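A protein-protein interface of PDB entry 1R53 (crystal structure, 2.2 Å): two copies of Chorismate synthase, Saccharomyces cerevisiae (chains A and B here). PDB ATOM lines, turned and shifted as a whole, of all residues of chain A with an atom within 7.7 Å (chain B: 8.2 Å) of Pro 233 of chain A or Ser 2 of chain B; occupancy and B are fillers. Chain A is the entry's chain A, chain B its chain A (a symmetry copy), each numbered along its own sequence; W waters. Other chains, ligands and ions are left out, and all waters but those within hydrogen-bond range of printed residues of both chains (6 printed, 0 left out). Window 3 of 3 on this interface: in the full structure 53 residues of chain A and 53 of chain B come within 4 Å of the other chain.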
ATOM      1  N   GLY A 229     -11.331   0.923  20.734  1.00  0.00           N
ATOM      2  CA  GLY A 229     -12.134   2.053  20.303  1.00  0.00           C
ATOM      3  C   GLY A 229     -13.292   1.732  19.390  1.00  0.00           C
ATOM      4  O   GLY A 229     -13.936   2.648  18.957  1.00  0.00           O
ATOM      5  N   LEU A 230     -13.625   0.470  19.115  1.00  0.00           N
ATOM      6  CA  LEU A 230     -14.732   0.218  18.192  1.00  0.00           C
ATOM      7  C   LEU A 230     -16.079   0.241  18.936  1.00  0.00           C
ATOM      8  O   LEU A 230     -16.173  -0.292  20.017  1.00  0.00           O
ATOM      9  CB  LEU A 230     -14.550  -1.099  17.460  1.00  0.00           C
ATOM     10  CG  LEU A 230     -13.639  -1.084  16.199  1.00  0.00           C
ATOM     11  CD1 LEU A 230     -12.285  -0.481  16.444  1.00  0.00           C
ATOM     12  CD2 LEU A 230     -13.459  -2.471  15.721  1.00  0.00           C
ATOM     13  N   GLY A 231     -17.117   0.797  18.309  1.00  0.00           N
ATOM     14  CA  GLY A 231     -18.419   0.976  18.916  1.00  0.00           C
ATOM     15  C   GLY A 231     -18.731   2.459  19.095  1.00  0.00           C
ATOM     16  O   GLY A 231     -17.825   3.286  19.176  1.00  0.00           O
ATOM     17  N   GLU A 232     -20.006   2.787  19.172  1.00  0.00           N
ATOM     18  CA  GLU A 232     -20.472   4.170  19.067  1.00  0.00           C
ATOM     19  C   GLU A 232     -21.589   4.477  20.075  1.00  0.00           C
ATOM     20  O   GLU A 232     -22.778   4.552  19.712  1.00  0.00           O
ATOM     21  CB  GLU A 232     -20.932   4.431  17.622  1.00  0.00           C
ATOM     22  CG  GLU A 232     -19.811   4.277  16.563  1.00  0.00           C
ATOM     23  CD  GLU A 232     -18.643   5.274  16.711  1.00  0.00           C
ATOM     24  OE1 GLU A 232     -18.969   6.427  17.003  1.00  0.00           O
ATOM     25  OE2 GLU A 232     -17.393   4.921  16.540  1.00  0.00           O
ATOM     26  N   PRO A 233     -21.205   4.667  21.331  1.00  0.00           N
ATOM     27  CA  PRO A 233     -22.151   5.040  22.402  1.00  0.00           C
ATOM     28  C   PRO A 233     -22.911   6.352  22.055  1.00  0.00           C
ATOM     29  O   PRO A 233     -22.452   7.103  21.182  1.00  0.00           O
ATOM     30  CB  PRO A 233     -21.255   5.209  23.651  1.00  0.00           C
ATOM     31  CG  PRO A 233     -19.867   4.829  23.276  1.00  0.00           C
ATOM     32  CD  PRO A 233     -19.809   4.573  21.819  1.00  0.00           C
ATOM     33  N   CYS A 234     -24.081   6.591  22.632  1.00  0.00           N
ATOM     34  CA  CYS A 234     -24.663   5.772  23.681  1.00  0.00           C
ATOM     35  C   CYS A 234     -25.607   4.680  23.158  1.00  0.00           C
ATOM     36  O   CYS A 234     -25.863   3.712  23.872  1.00  0.00           O
ATOM     37  CB  CYS A 234     -25.379   6.691  24.663  1.00  0.00           C
ATOM     38  SG  CYS A 234     -26.880   7.496  24.004  1.00  0.00           S
ATOM     39  N   PHE A 235     -26.094   4.786  21.916  1.00  0.00           N
ATOM     40  CA  PHE A 235     -27.060   3.811  21.437  1.00  0.00           C
ATOM     41  C   PHE A 235     -26.510   2.730  20.507  1.00  0.00           C
ATOM     42  O   PHE A 235     -27.117   1.681  20.408  1.00  0.00           O
ATOM     43  CB  PHE A 235     -28.223   4.464  20.731  1.00  0.00           C
ATOM     44  CG  PHE A 235     -29.129   5.258  21.624  1.00  0.00           C
ATOM     45  CD1 PHE A 235     -29.909   4.629  22.610  1.00  0.00           C
ATOM     46  CD2 PHE A 235     -29.263   6.634  21.448  1.00  0.00           C
ATOM     47  CE1 PHE A 235     -30.752   5.366  23.453  1.00  0.00           C
ATOM     48  CE2 PHE A 235     -30.148   7.397  22.285  1.00  0.00           C
ATOM     49  CZ  PHE A 235     -30.898   6.763  23.271  1.00  0.00           C
ATOM     50  N   ASP A 236     -25.432   3.008  19.786  1.00  0.00           N
ATOM     51  CA  ASP A 236     -24.775   2.044  18.926  1.00  0.00           C
ATOM     52  C   ASP A 236     -23.465   1.531  19.501  1.00  0.00           C
ATOM     53  O   ASP A 236     -22.490   1.341  18.779  1.00  0.00           O
ATOM     54  CB  ASP A 236     -24.573   2.653  17.553  1.00  0.00           C
ATOM     55  CG  ASP A 236     -25.874   3.209  17.004  1.00  0.00           C
ATOM     56  OD1 ASP A 236     -26.932   2.628  17.315  1.00  0.00           O
ATOM     57  OD2 ASP A 236     -25.951   4.258  16.316  1.00  0.00           O
ATOM     58  N   LYS A 237     -23.475   1.288  20.804  1.00  0.00           N
ATOM     59  CA  LYS A 237     -22.402   0.558  21.502  1.00  0.00           C
ATOM     60  C   LYS A 237     -22.146  -0.732  20.761  1.00  0.00           C
ATOM     61  O   LYS A 237     -23.020  -1.265  20.128  1.00  0.00           O
ATOM     62  CB  LYS A 237     -22.832   0.222  22.902  1.00  0.00           C
ATOM     63  CG  LYS A 237     -23.210   1.407  23.760  1.00  0.00           C
ATOM     64  CD  LYS A 237     -23.498   0.968  25.227  1.00  0.00           C
ATOM     65  CE  LYS A 237     -23.606   2.205  26.132  1.00  0.00           C
ATOM     66  NZ  LYS A 237     -24.182   1.876  27.485  1.00  0.00           N
ATOM     67  N   LEU A 238     -20.925  -1.211  20.780  1.00  0.00           N
ATOM     68  CA  LEU A 238     -20.573  -2.378  19.966  1.00  0.00           C
ATOM     69  C   LEU A 238     -21.458  -3.605  20.295  1.00  0.00           C
ATOM     70  O   LEU A 238     -21.884  -4.331  19.402  1.00  0.00           O
ATOM     71  CB  LEU A 238     -19.073  -2.682  20.158  1.00  0.00           C
ATOM     72  CG  LEU A 238     -18.482  -3.752  19.237  1.00  0.00           C
ATOM     73  CD1 LEU A 238     -18.619  -3.310  17.750  1.00  0.00           C
ATOM     74  CD2 LEU A 238     -17.080  -3.985  19.567  1.00  0.00           C
ATOM     75  N   GLU A 239     -21.743  -3.831  21.585  1.00  0.00           N
ATOM     76  CA  GLU A 239     -22.535  -4.978  21.993  1.00  0.00           C
ATOM     77  C   GLU A 239     -23.986  -4.847  21.499  1.00  0.00           C
ATOM     78  O   GLU A 239     -24.653  -5.849  21.293  1.00  0.00           O
ATOM     79  CB  GLU A 239     -22.484  -5.193  23.504  1.00  0.00           C
ATOM     80  CG  GLU A 239     -22.971  -4.048  24.378  1.00  0.00           C
ATOM     81  CD  GLU A 239     -21.822  -3.185  24.894  1.00  0.00           C
ATOM     82  OE1 GLU A 239     -20.983  -2.707  24.088  1.00  0.00           O
ATOM     83  OE2 GLU A 239     -21.738  -3.011  26.110  1.00  0.00           O
ATOM     84  N   MET A 241     -24.758  -3.231  18.600  1.00  0.00           N
ATOM     85  CA  MET A 241     -24.673  -3.527  17.161  1.00  0.00           C
ATOM     86  C   MET A 241     -24.584  -5.046  16.993  1.00  0.00           C
ATOM     87  O   MET A 241     -25.214  -5.608  16.129  1.00  0.00           O
ATOM     88  CB  MET A 241     -23.471  -2.829  16.481  1.00  0.00           C
ATOM     89  CG  MET A 241     -23.385  -1.190  16.557  1.00  0.00           C
ATOM     90  SD  MET A 241     -21.724  -0.564  16.171  1.00  0.00           S
ATOM     91  CE  MET A 241     -21.818  -0.969  14.620  1.00  0.00           C
ATOM     92  N   GLN A 295     -15.918  -2.092  27.136  1.00  0.00           N
ATOM     93  CA  GLN A 295     -16.097  -1.229  28.311  1.00  0.00           C
ATOM     94  C   GLN A 295     -16.724   0.062  27.815  1.00  0.00           C
ATOM     95  O   GLN A 295     -16.236   0.650  26.831  1.00  0.00           O
ATOM     96  CB  GLN A 295     -14.751  -0.816  28.950  1.00  0.00           C
ATOM     97  CG  GLN A 295     -14.119  -1.757  29.980  1.00  0.00           C
ATOM     98  CD  GLN A 295     -12.615  -1.414  30.214  1.00  0.00           C
ATOM     99  OE1 GLN A 295     -12.276  -0.221  30.387  1.00  0.00           O
ATOM    100  NE2 GLN A 295     -11.727  -2.439  30.170  1.00  0.00           N
ATOM    101  N   GLY A 296     -17.742   0.537  28.523  1.00  0.00           N
ATOM    102  CA  GLY A 296     -18.501   1.687  28.086  1.00  0.00           C
ATOM    103  C   GLY A 296     -19.013   1.584  26.662  1.00  0.00           C
ATOM    104  O   GLY A 296     -19.127   2.595  25.949  1.00  0.00           O
ATOM    105  N   GLY A 297     -19.277   0.376  26.189  1.00  0.00           N
ATOM    106  CA  GLY A 297     -19.787   0.224  24.845  1.00  0.00           C
ATOM    107  C   GLY A 297     -18.756   0.276  23.746  1.00  0.00           C
ATOM    108  O   GLY A 297     -19.108   0.298  22.568  1.00  0.00           O
ATOM    109  N   ILE A 298     -17.478   0.308  24.078  1.00  0.00           N
ATOM    110  CA  ILE A 298     -16.465   0.233  23.024  1.00  0.00           C
ATOM    111  C   ILE A 298     -15.454  -0.880  23.267  1.00  0.00           C
ATOM    112  O   ILE A 298     -15.188  -1.246  24.421  1.00  0.00           O
ATOM    113  CB  ILE A 298     -15.755   1.597  22.834  1.00  0.00           C
ATOM    114  CG1 ILE A 298     -14.913   1.942  24.038  1.00  0.00           C
ATOM    115  CG2 ILE A 298     -16.783   2.728  22.611  1.00  0.00           C
ATOM    116  CD1 ILE A 298     -13.961   3.077  23.740  1.00  0.00           C
ATOM    117  N   ARG A 368     -13.211   8.960  12.909  1.00  0.00           N
ATOM    118  CA  ARG A 368     -12.995   9.952  13.955  1.00  0.00           C
ATOM    119  C   ARG A 368     -11.640   9.854  14.660  1.00  0.00           C
ATOM    120  O   ARG A 368     -11.381  10.618  15.552  1.00  0.00           O
ATOM    121  CB  ARG A 368     -14.154   9.916  14.961  1.00  0.00           C
ATOM    122  CG  ARG A 368     -15.548  10.048  14.275  1.00  0.00           C
ATOM    123  CD  ARG A 368     -16.604  10.868  15.072  1.00  0.00           C
ATOM    124  NE  ARG A 368     -17.989  10.760  14.561  1.00  0.00           N
ATOM    125  CZ  ARG A 368     -18.748   9.673  14.689  1.00  0.00           C
ATOM    126  NH1 ARG A 368     -18.274   8.595  15.275  1.00  0.00           N
ATOM    127  NH2 ARG A 368     -19.984   9.647  14.248  1.00  0.00           N
ATOM    128  N   MET B   1     -24.278   6.269  17.578  1.00  0.00           N
ATOM    129  CA  MET B   1     -24.141   7.580  18.286  1.00  0.00           C
ATOM    130  C   MET B   1     -25.299   7.704  19.285  1.00  0.00           C
ATOM    131  O   MET B   1     -25.807   6.689  19.767  1.00  0.00           O
ATOM    132  N   SER B   2     -25.721   8.921  19.562  1.00  0.00           N
ATOM    133  CA  SER B   2     -26.715   9.194  20.590  1.00  0.00           C
ATOM    134  C   SER B   2     -28.092   9.545  20.038  1.00  0.00           C
ATOM    135  O   SER B   2     -28.950  10.042  20.748  1.00  0.00           O
ATOM    136  CB  SER B   2     -26.188  10.233  21.585  1.00  0.00           C
ATOM    137  OG  SER B   2     -25.037   9.689  22.313  1.00  0.00           O
ATOM    138  N   THR B   3     -28.337   9.151  18.802  1.00  0.00           N
ATOM    139  CA  THR B   3     -29.706   9.084  18.254  1.00  0.00           C
ATOM    140  C   THR B   3     -30.226   7.648  18.137  1.00  0.00           C
ATOM    141  O   THR B   3     -29.500   6.745  17.693  1.00  0.00           O
ATOM    142  CB  THR B   3     -29.751   9.773  16.846  1.00  0.00           C
ATOM    143  OG1 THR B   3     -29.489  11.159  17.010  1.00  0.00           O
ATOM    144  CG2 THR B   3     -31.160   9.747  16.263  1.00  0.00           C
ATOM    145  N   PHE B   4     -31.486   7.458  18.525  1.00  0.00           N
ATOM    146  CA  PHE B   4     -32.156   6.175  18.528  1.00  0.00           C
ATOM    147  C   PHE B   4     -33.474   6.309  17.789  1.00  0.00           C
ATOM    148  O   PHE B   4     -34.226   7.273  18.016  1.00  0.00           O
ATOM    149  CB  PHE B   4     -32.435   5.705  19.965  1.00  0.00           C
ATOM    150  CG  PHE B   4     -32.992   4.286  20.044  1.00  0.00           C
ATOM    151  CD1 PHE B   4     -32.158   3.207  19.948  1.00  0.00           C
ATOM    152  CD2 PHE B   4     -34.356   4.055  20.160  1.00  0.00           C
ATOM    153  CE1 PHE B   4     -32.664   1.919  19.975  1.00  0.00           C
ATOM    154  CE2 PHE B   4     -34.877   2.753  20.187  1.00  0.00           C
ATOM    155  CZ  PHE B   4     -34.027   1.695  20.083  1.00  0.00           C
ATOM    156  N   GLY B   5     -33.765   5.367  16.912  1.00  0.00           N
ATOM    157  CA  GLY B   5     -34.998   5.373  16.156  1.00  0.00           C
ATOM    158  C   GLY B   5     -34.904   5.897  14.745  1.00  0.00           C
ATOM    159  O   GLY B   5     -33.974   6.617  14.393  1.00  0.00           O
ATOM    160  N   ARG B   9     -37.844   9.328  17.019  1.00  0.00           N
ATOM    161  CA  ARG B   9     -36.418   9.518  17.202  1.00  0.00           C
ATOM    162  C   ARG B   9     -36.145  10.224  18.505  1.00  0.00           C
ATOM    163  O   ARG B   9     -36.884  11.143  18.863  1.00  0.00           O
ATOM    164  CB  ARG B   9     -35.858  10.359  16.046  1.00  0.00           C
ATOM    165  CG  ARG B   9     -35.579   9.613  14.744  1.00  0.00           C
ATOM    166  CD  ARG B   9     -34.990  10.477  13.610  1.00  0.00           C
ATOM    167  NE  ARG B   9     -35.953  11.559  13.319  1.00  0.00           N
ATOM    168  CZ  ARG B   9     -36.962  11.543  12.415  1.00  0.00           C
ATOM    169  NH1 ARG B   9     -37.777  12.577  12.348  1.00  0.00           N
ATOM    170  NH2 ARG B   9     -37.171  10.532  11.580  1.00  0.00           N
ATOM    171  N   VAL B  10     -35.127   9.794  19.240  1.00  0.00           N
ATOM    172  CA  VAL B  10     -34.608  10.581  20.356  1.00  0.00           C
ATOM    173  C   VAL B  10     -33.109  10.750  20.234  1.00  0.00           C
ATOM    174  O   VAL B  10     -32.403   9.794  19.943  1.00  0.00           O
ATOM    175  CB  VAL B  10     -34.994  10.015  21.786  1.00  0.00           C
ATOM    176  CG1 VAL B  10     -34.532   8.599  21.980  1.00  0.00           C
ATOM    177  CG2 VAL B  10     -34.422  10.896  22.866  1.00  0.00           C
ATOM    178  N   THR B  11     -32.648  11.989  20.427  1.00  0.00           N
ATOM    179  CA  THR B  11     -31.246  12.295  20.504  1.00  0.00           C
ATOM    180  C   THR B  11     -31.010  12.774  21.938  1.00  0.00           C
ATOM    181  O   THR B  11     -31.687  13.682  22.412  1.00  0.00           O
ATOM    182  CB  THR B  11     -30.904  13.371  19.493  1.00  0.00           C
ATOM    183  OG1 THR B  11     -31.249  12.951  18.155  1.00  0.00           O
ATOM    184  CG2 THR B  11     -29.365  13.647  19.446  1.00  0.00           C
ATOM    185  N   THR B  12     -30.049  12.175  22.632  1.00  0.00           N
ATOM    186  CA  THR B  12     -29.793  12.500  24.036  1.00  0.00           C
ATOM    187  C   THR B  12     -28.494  13.233  24.202  1.00  0.00           C
ATOM    188  O   THR B  12     -27.699  13.300  23.258  1.00  0.00           O
ATOM    189  CB  THR B  12     -29.823  11.233  24.899  1.00  0.00           C
ATOM    190  OG1 THR B  12     -28.785  10.306  24.521  1.00  0.00           O
ATOM    191  CG2 THR B  12     -31.117  10.490  24.683  1.00  0.00           C
ATOM    192  N   TYR B  13     -28.304  13.807  25.393  1.00  0.00           N
ATOM    193  CA  TYR B  13     -27.076  14.514  25.779  1.00  0.00           C
ATOM    194  C   TYR B  13     -26.912  14.505  27.317  1.00  0.00           C
ATOM    195  O   TYR B  13     -27.877  14.356  28.028  1.00  0.00           O
ATOM    196  CB  TYR B  13     -27.038  15.975  25.234  1.00  0.00           C
ATOM    197  CG  TYR B  13     -27.901  17.010  25.977  1.00  0.00           C
ATOM    198  CD1 TYR B  13     -27.399  17.747  27.055  1.00  0.00           C
ATOM    199  CD2 TYR B  13     -29.214  17.243  25.600  1.00  0.00           C
ATOM    200  CE1 TYR B  13     -28.196  18.705  27.708  1.00  0.00           C
ATOM    201  CE2 TYR B  13     -30.000  18.154  26.247  1.00  0.00           C
ATOM    202  CZ  TYR B  13     -29.486  18.899  27.297  1.00  0.00           C
ATOM    203  OH  TYR B  13     -30.294  19.809  27.928  1.00  0.00           O
ATOM    204  N   GLY B  14     -25.682  14.684  27.803  1.00  0.00           N
ATOM    205  CA  GLY B  14     -25.418  14.792  29.234  1.00  0.00           C
ATOM    206  C   GLY B  14     -24.391  13.821  29.778  1.00  0.00           C
ATOM    207  O   GLY B  14     -24.484  12.627  29.503  1.00  0.00           O
ATOM    208  N   GLY B  22     -30.450  15.973  28.866  1.00  0.00           N
ATOM    209  CA  GLY B  22     -31.739  16.028  28.213  1.00  0.00           C
ATOM    210  C   GLY B  22     -31.775  15.265  26.924  1.00  0.00           C
ATOM    211  O   GLY B  22     -30.946  14.392  26.692  1.00  0.00           O
ATOM    212  N   CYS B  23     -32.735  15.632  26.085  1.00  0.00           N
ATOM    213  CA  CYS B  23     -32.936  14.994  24.816  1.00  0.00           C
ATOM    214  C   CYS B  23     -33.829  15.804  23.918  1.00  0.00           C
ATOM    215  O   CYS B  23     -34.549  16.718  24.382  1.00  0.00           O
ATOM    216  CB  CYS B  23     -33.590  13.640  25.040  1.00  0.00           C
ATOM    217  SG  CYS B  23     -35.214  13.768  25.839  1.00  0.00           S
ATOM    218  N   ILE B  24     -33.828  15.431  22.640  1.00  0.00           N
ATOM    219  CA  ILE B  24     -34.746  15.981  21.653  1.00  0.00           C
ATOM    220  C   ILE B  24     -35.505  14.814  21.056  1.00  0.00           C
ATOM    221  O   ILE B  24     -34.891  13.872  20.560  1.00  0.00           O
ATOM    222  CB  ILE B  24     -33.980  16.752  20.544  1.00  0.00           C
ATOM    223  CG1 ILE B  24     -33.244  17.952  21.133  1.00  0.00           C
ATOM    224  CG2 ILE B  24     -34.948  17.193  19.438  1.00  0.00           C
ATOM    225  CD1 ILE B  24     -32.297  18.641  20.194  1.00  0.00           C
ATOM    226  N   ARG B 127     -21.923   9.102  31.082  1.00  0.00           N
ATOM    227  CA  ARG B 127     -23.214   9.463  30.477  1.00  0.00           C
ATOM    228  C   ARG B 127     -24.386   9.265  31.459  1.00  0.00           C
ATOM    229  O   ARG B 127     -24.189   8.739  32.562  1.00  0.00           O
ATOM    230  CB  ARG B 127     -23.450   8.669  29.167  1.00  0.00           C
ATOM    231  N   ARG B 132     -33.299   9.058  28.020  1.00  0.00           N
ATOM    232  CA  ARG B 132     -33.999   7.859  27.632  1.00  0.00           C
ATOM    233  C   ARG B 132     -35.333   7.721  28.326  1.00  0.00           C
ATOM    234  O   ARG B 132     -36.331   7.395  27.687  1.00  0.00           O
ATOM    235  CB  ARG B 132     -33.188   6.600  27.954  1.00  0.00           C
ATOM    236  CG  ARG B 132     -31.868   6.469  27.216  1.00  0.00           C
ATOM    237  CD  ARG B 132     -31.016   5.430  27.834  1.00  0.00           C
ATOM    238  NE  ARG B 132     -29.661   5.339  27.294  1.00  0.00           N
ATOM    239  CZ  ARG B 132     -29.195   4.294  26.607  1.00  0.00           C
ATOM    240  NH1 ARG B 132     -29.983   3.246  26.287  1.00  0.00           N
ATOM    241  NH2 ARG B 132     -27.937   4.312  26.189  1.00  0.00           N
ATOM    242  N   SER B 248     -27.867  -1.453  24.715  1.00  0.00           N
ATOM    243  CA  SER B 248     -27.357  -0.114  24.931  1.00  0.00           C
ATOM    244  C   SER B 248     -27.481   0.399  26.360  1.00  0.00           C
ATOM    245  O   SER B 248     -26.890   1.414  26.664  1.00  0.00           O
ATOM    246  CB  SER B 248     -28.028   0.870  23.979  1.00  0.00           C
ATOM    247  OG  SER B 248     -29.292   1.271  24.434  1.00  0.00           O
HETATM  248  O   HOH W   1     -25.560  10.765  25.402  1.00  0.00           O
HETATM  249  O   HOH W   2     -28.673   8.509  26.825  1.00  0.00           O
HETATM  250  O   HOH W   3     -29.321   3.812  17.167  1.00  0.00           O
HETATM  251  O   HOH W   4     -27.061   7.457  16.655  1.00  0.00           O
HETATM  252  O   HOH W   5     -22.731   9.942  20.980  1.00  0.00           O
HETATM  253  O   HOH W   6     -23.237   5.320  15.063  1.00  0.00           O
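The backbone carbonyl oxygen (O) of Glu 232 of chain A lies within hydrogen-bond range of the backbone NH (N) of Met 1 of chain B. The backbone NH (N) of Cys 234 of chain A lies within hydrogen-bond range of the backbone carbonyl oxygen (O) of Met 1 of chain B (3.3 Å). The backbone NH of Cys 234 of chain A sits at hydrogen-bond distance from the side-chain hydroxyl of Ser 2 of chain B, 3.3 Å away. The side-chain sulfur (SG) of Cys 234 of chain A lies within hydrogen-bond range of the side-chain hydroxyl (OG1) of Thr 12 of chain B (3.4 Å). O of Cys 234 of chain A sits at hydrogen-bond distance from NH2 of Arg 132 of chain B, at 3.2 Å. The backbone NH (N) of Phe 235 of chain A is in hydrogen-bond range of the backbone carbonyl oxygen (O) of Met 1 of chain B. The side-chain carboxylate of Asp 236 of chain A lies within hydrogen-bond range of the backbone NH of Met 1 of chain B (2.9 Å). The side-chain amino group of Lys 237 of chain A sits at hydrogen-bond distance from the backbone carbonyl oxygen of Ser 248 of chain B (2.9 Å).
OE1 of Glu 232 of chain A lies within salt-bridge range of NH1 of Arg 368 of chain A, 2.9 Å away. N of Thr 12 of chain B sits at hydrogen-bond distance from O of Ser 2 of chain B. OG1 of Thr 3 of chain B lies within hydrogen-bond range of OG1 of Thr 11 of chain B, 2.8 Å away. N of Phe 4 of chain B lies within hydrogen-bond range of O of Val 10 of chain B, at 2.9 Å. NH1 of Arg 132 of chain B lies within hydrogen-bond range of OG of Ser 248 of chain B (2.8 Å).
Among the printed residues, merely in contact across the chains: Phe 235 of chain A with Ser 2 of chain B, Pro 233 of chain A with Met 1 of chain B, Cys 234 of chain A with Ser 248 of chain B, Phe 235 of chain A with Thr 3 of chain B, Phe 235 of chain A with Arg 132 of chain B, Phe 235 of chain A with Phe 4 of chain B, Phe 235 of chain A with Ser 248 of chain B, Pro 233 of chain A with Ser 2 of chain B and Phe 235 of chain A with Thr 12 of chain B.
Of chain B, only Met 1 (3.4 Å) and Ser 2 (3.8 Å) come within 4 Å of Pro 233 of chain A. Ser 2 of chain B touches three residues of chain A. Printed residues of chain A within 4 Å of Met 1 of chain B: Glu 232 (3.1 Å), Pro 233 (3.4 Å), Cys 234 (3.3 Å), Phe 235 (2.9 Å) and Asp 236 (2.9 Å). Printed residues of chain A within 4 Å of Thr 12 of chain B: Cys 234 and Phe 235. Of the printed residues of chain A, Phe 4 of chain B touches Phe 235 (3.6 Å). Of the printed residues of chain A, Arg 132 of chain B touches Cys 234 and Phe 235. Of the printed residues of chain B, Glu 232 of chain A touches Met 1 (3.1 Å). Printed residues of chain B within 4 Å of Lys 237 of chain A: Ser 248. Leu 230 of chain A touches none of the printed residues of chain B. The nearest residue of chain B that does not touch Pro 233 of chain A is Thr 3 of chain B (6.7 Å). The nearest residue of chain A that does not touch Ser 2 of chain B is Glu 232 of chain A (5.3 Å). The nearest printed residue of chain B that does not touch Phe 235 of chain A is Val 10 of chain B (4.04 Å).
Of the 17 printed residues of chain A, 6 touch a printed residue of chain B. Hydrophobic or aromatic side chains of chain A that line the printed part of chain B: Phe 235. Printed residues of chain B that touch a printed residue of chain A: Met 1, Ser 2, Thr 3, Phe 4, Thr 12, Arg 132 and Ser 248. Hydrophobic or aromatic side chains of chain B that line the printed part of chain A: Phe 4. Among the printed residues, no Asp or Glu carboxylate lies within 4 Å of a Lys or Arg side-chain nitrogen of the other chain.
No position is printed for both chains. Of the 17 pairs that touch across the chains among the printed residues, none has its exchanged pair printed and touching as well.
Water W3 lies within hydrogen-bond range of the side-chain carboxylate of Asp 236 of chain A (2.7 Å) and the backbone carbonyl oxygen of Thr 3 of chain B (3.0 Å). Water W5 bridges OG of Ser 2 of chain B (2.7 Å) and O of Pro 233 of chain A (2.9 Å). Water W4 lies within hydrogen-bond range of the backbone carbonyl oxygen (O) of Thr 3 of chain B (2.7 Å), the backbone NH (N) of Met 1 of chain B (3.2 Å) and the side-chain carboxylate (OD2) of Asp 236 of chain A (3.4 Å). Water W6 bridges N of Met 1 of chain B (2.9 Å) and OD2 of Asp 236 of chain A (3.2 Å). Water W2 lies within hydrogen-bond range of the side-chain hydroxyl of Thr 12 of chain B (2.9 Å), the guanidinium group of Arg 132 of chain B (3.4 Å) and the side-chain sulfur of Cys 234 of chain A (3.5 Å). Water W1 lies within hydrogen-bond range of the side-chain hydroxyl (OG) of Ser 2 of chain B (3.3 Å), the side-chain hydroxyl (OG1) of Thr 12 of chain B (3.4 Å) and the side-chain sulfur (SG) of Cys 234 of chain A (3.8 Å).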
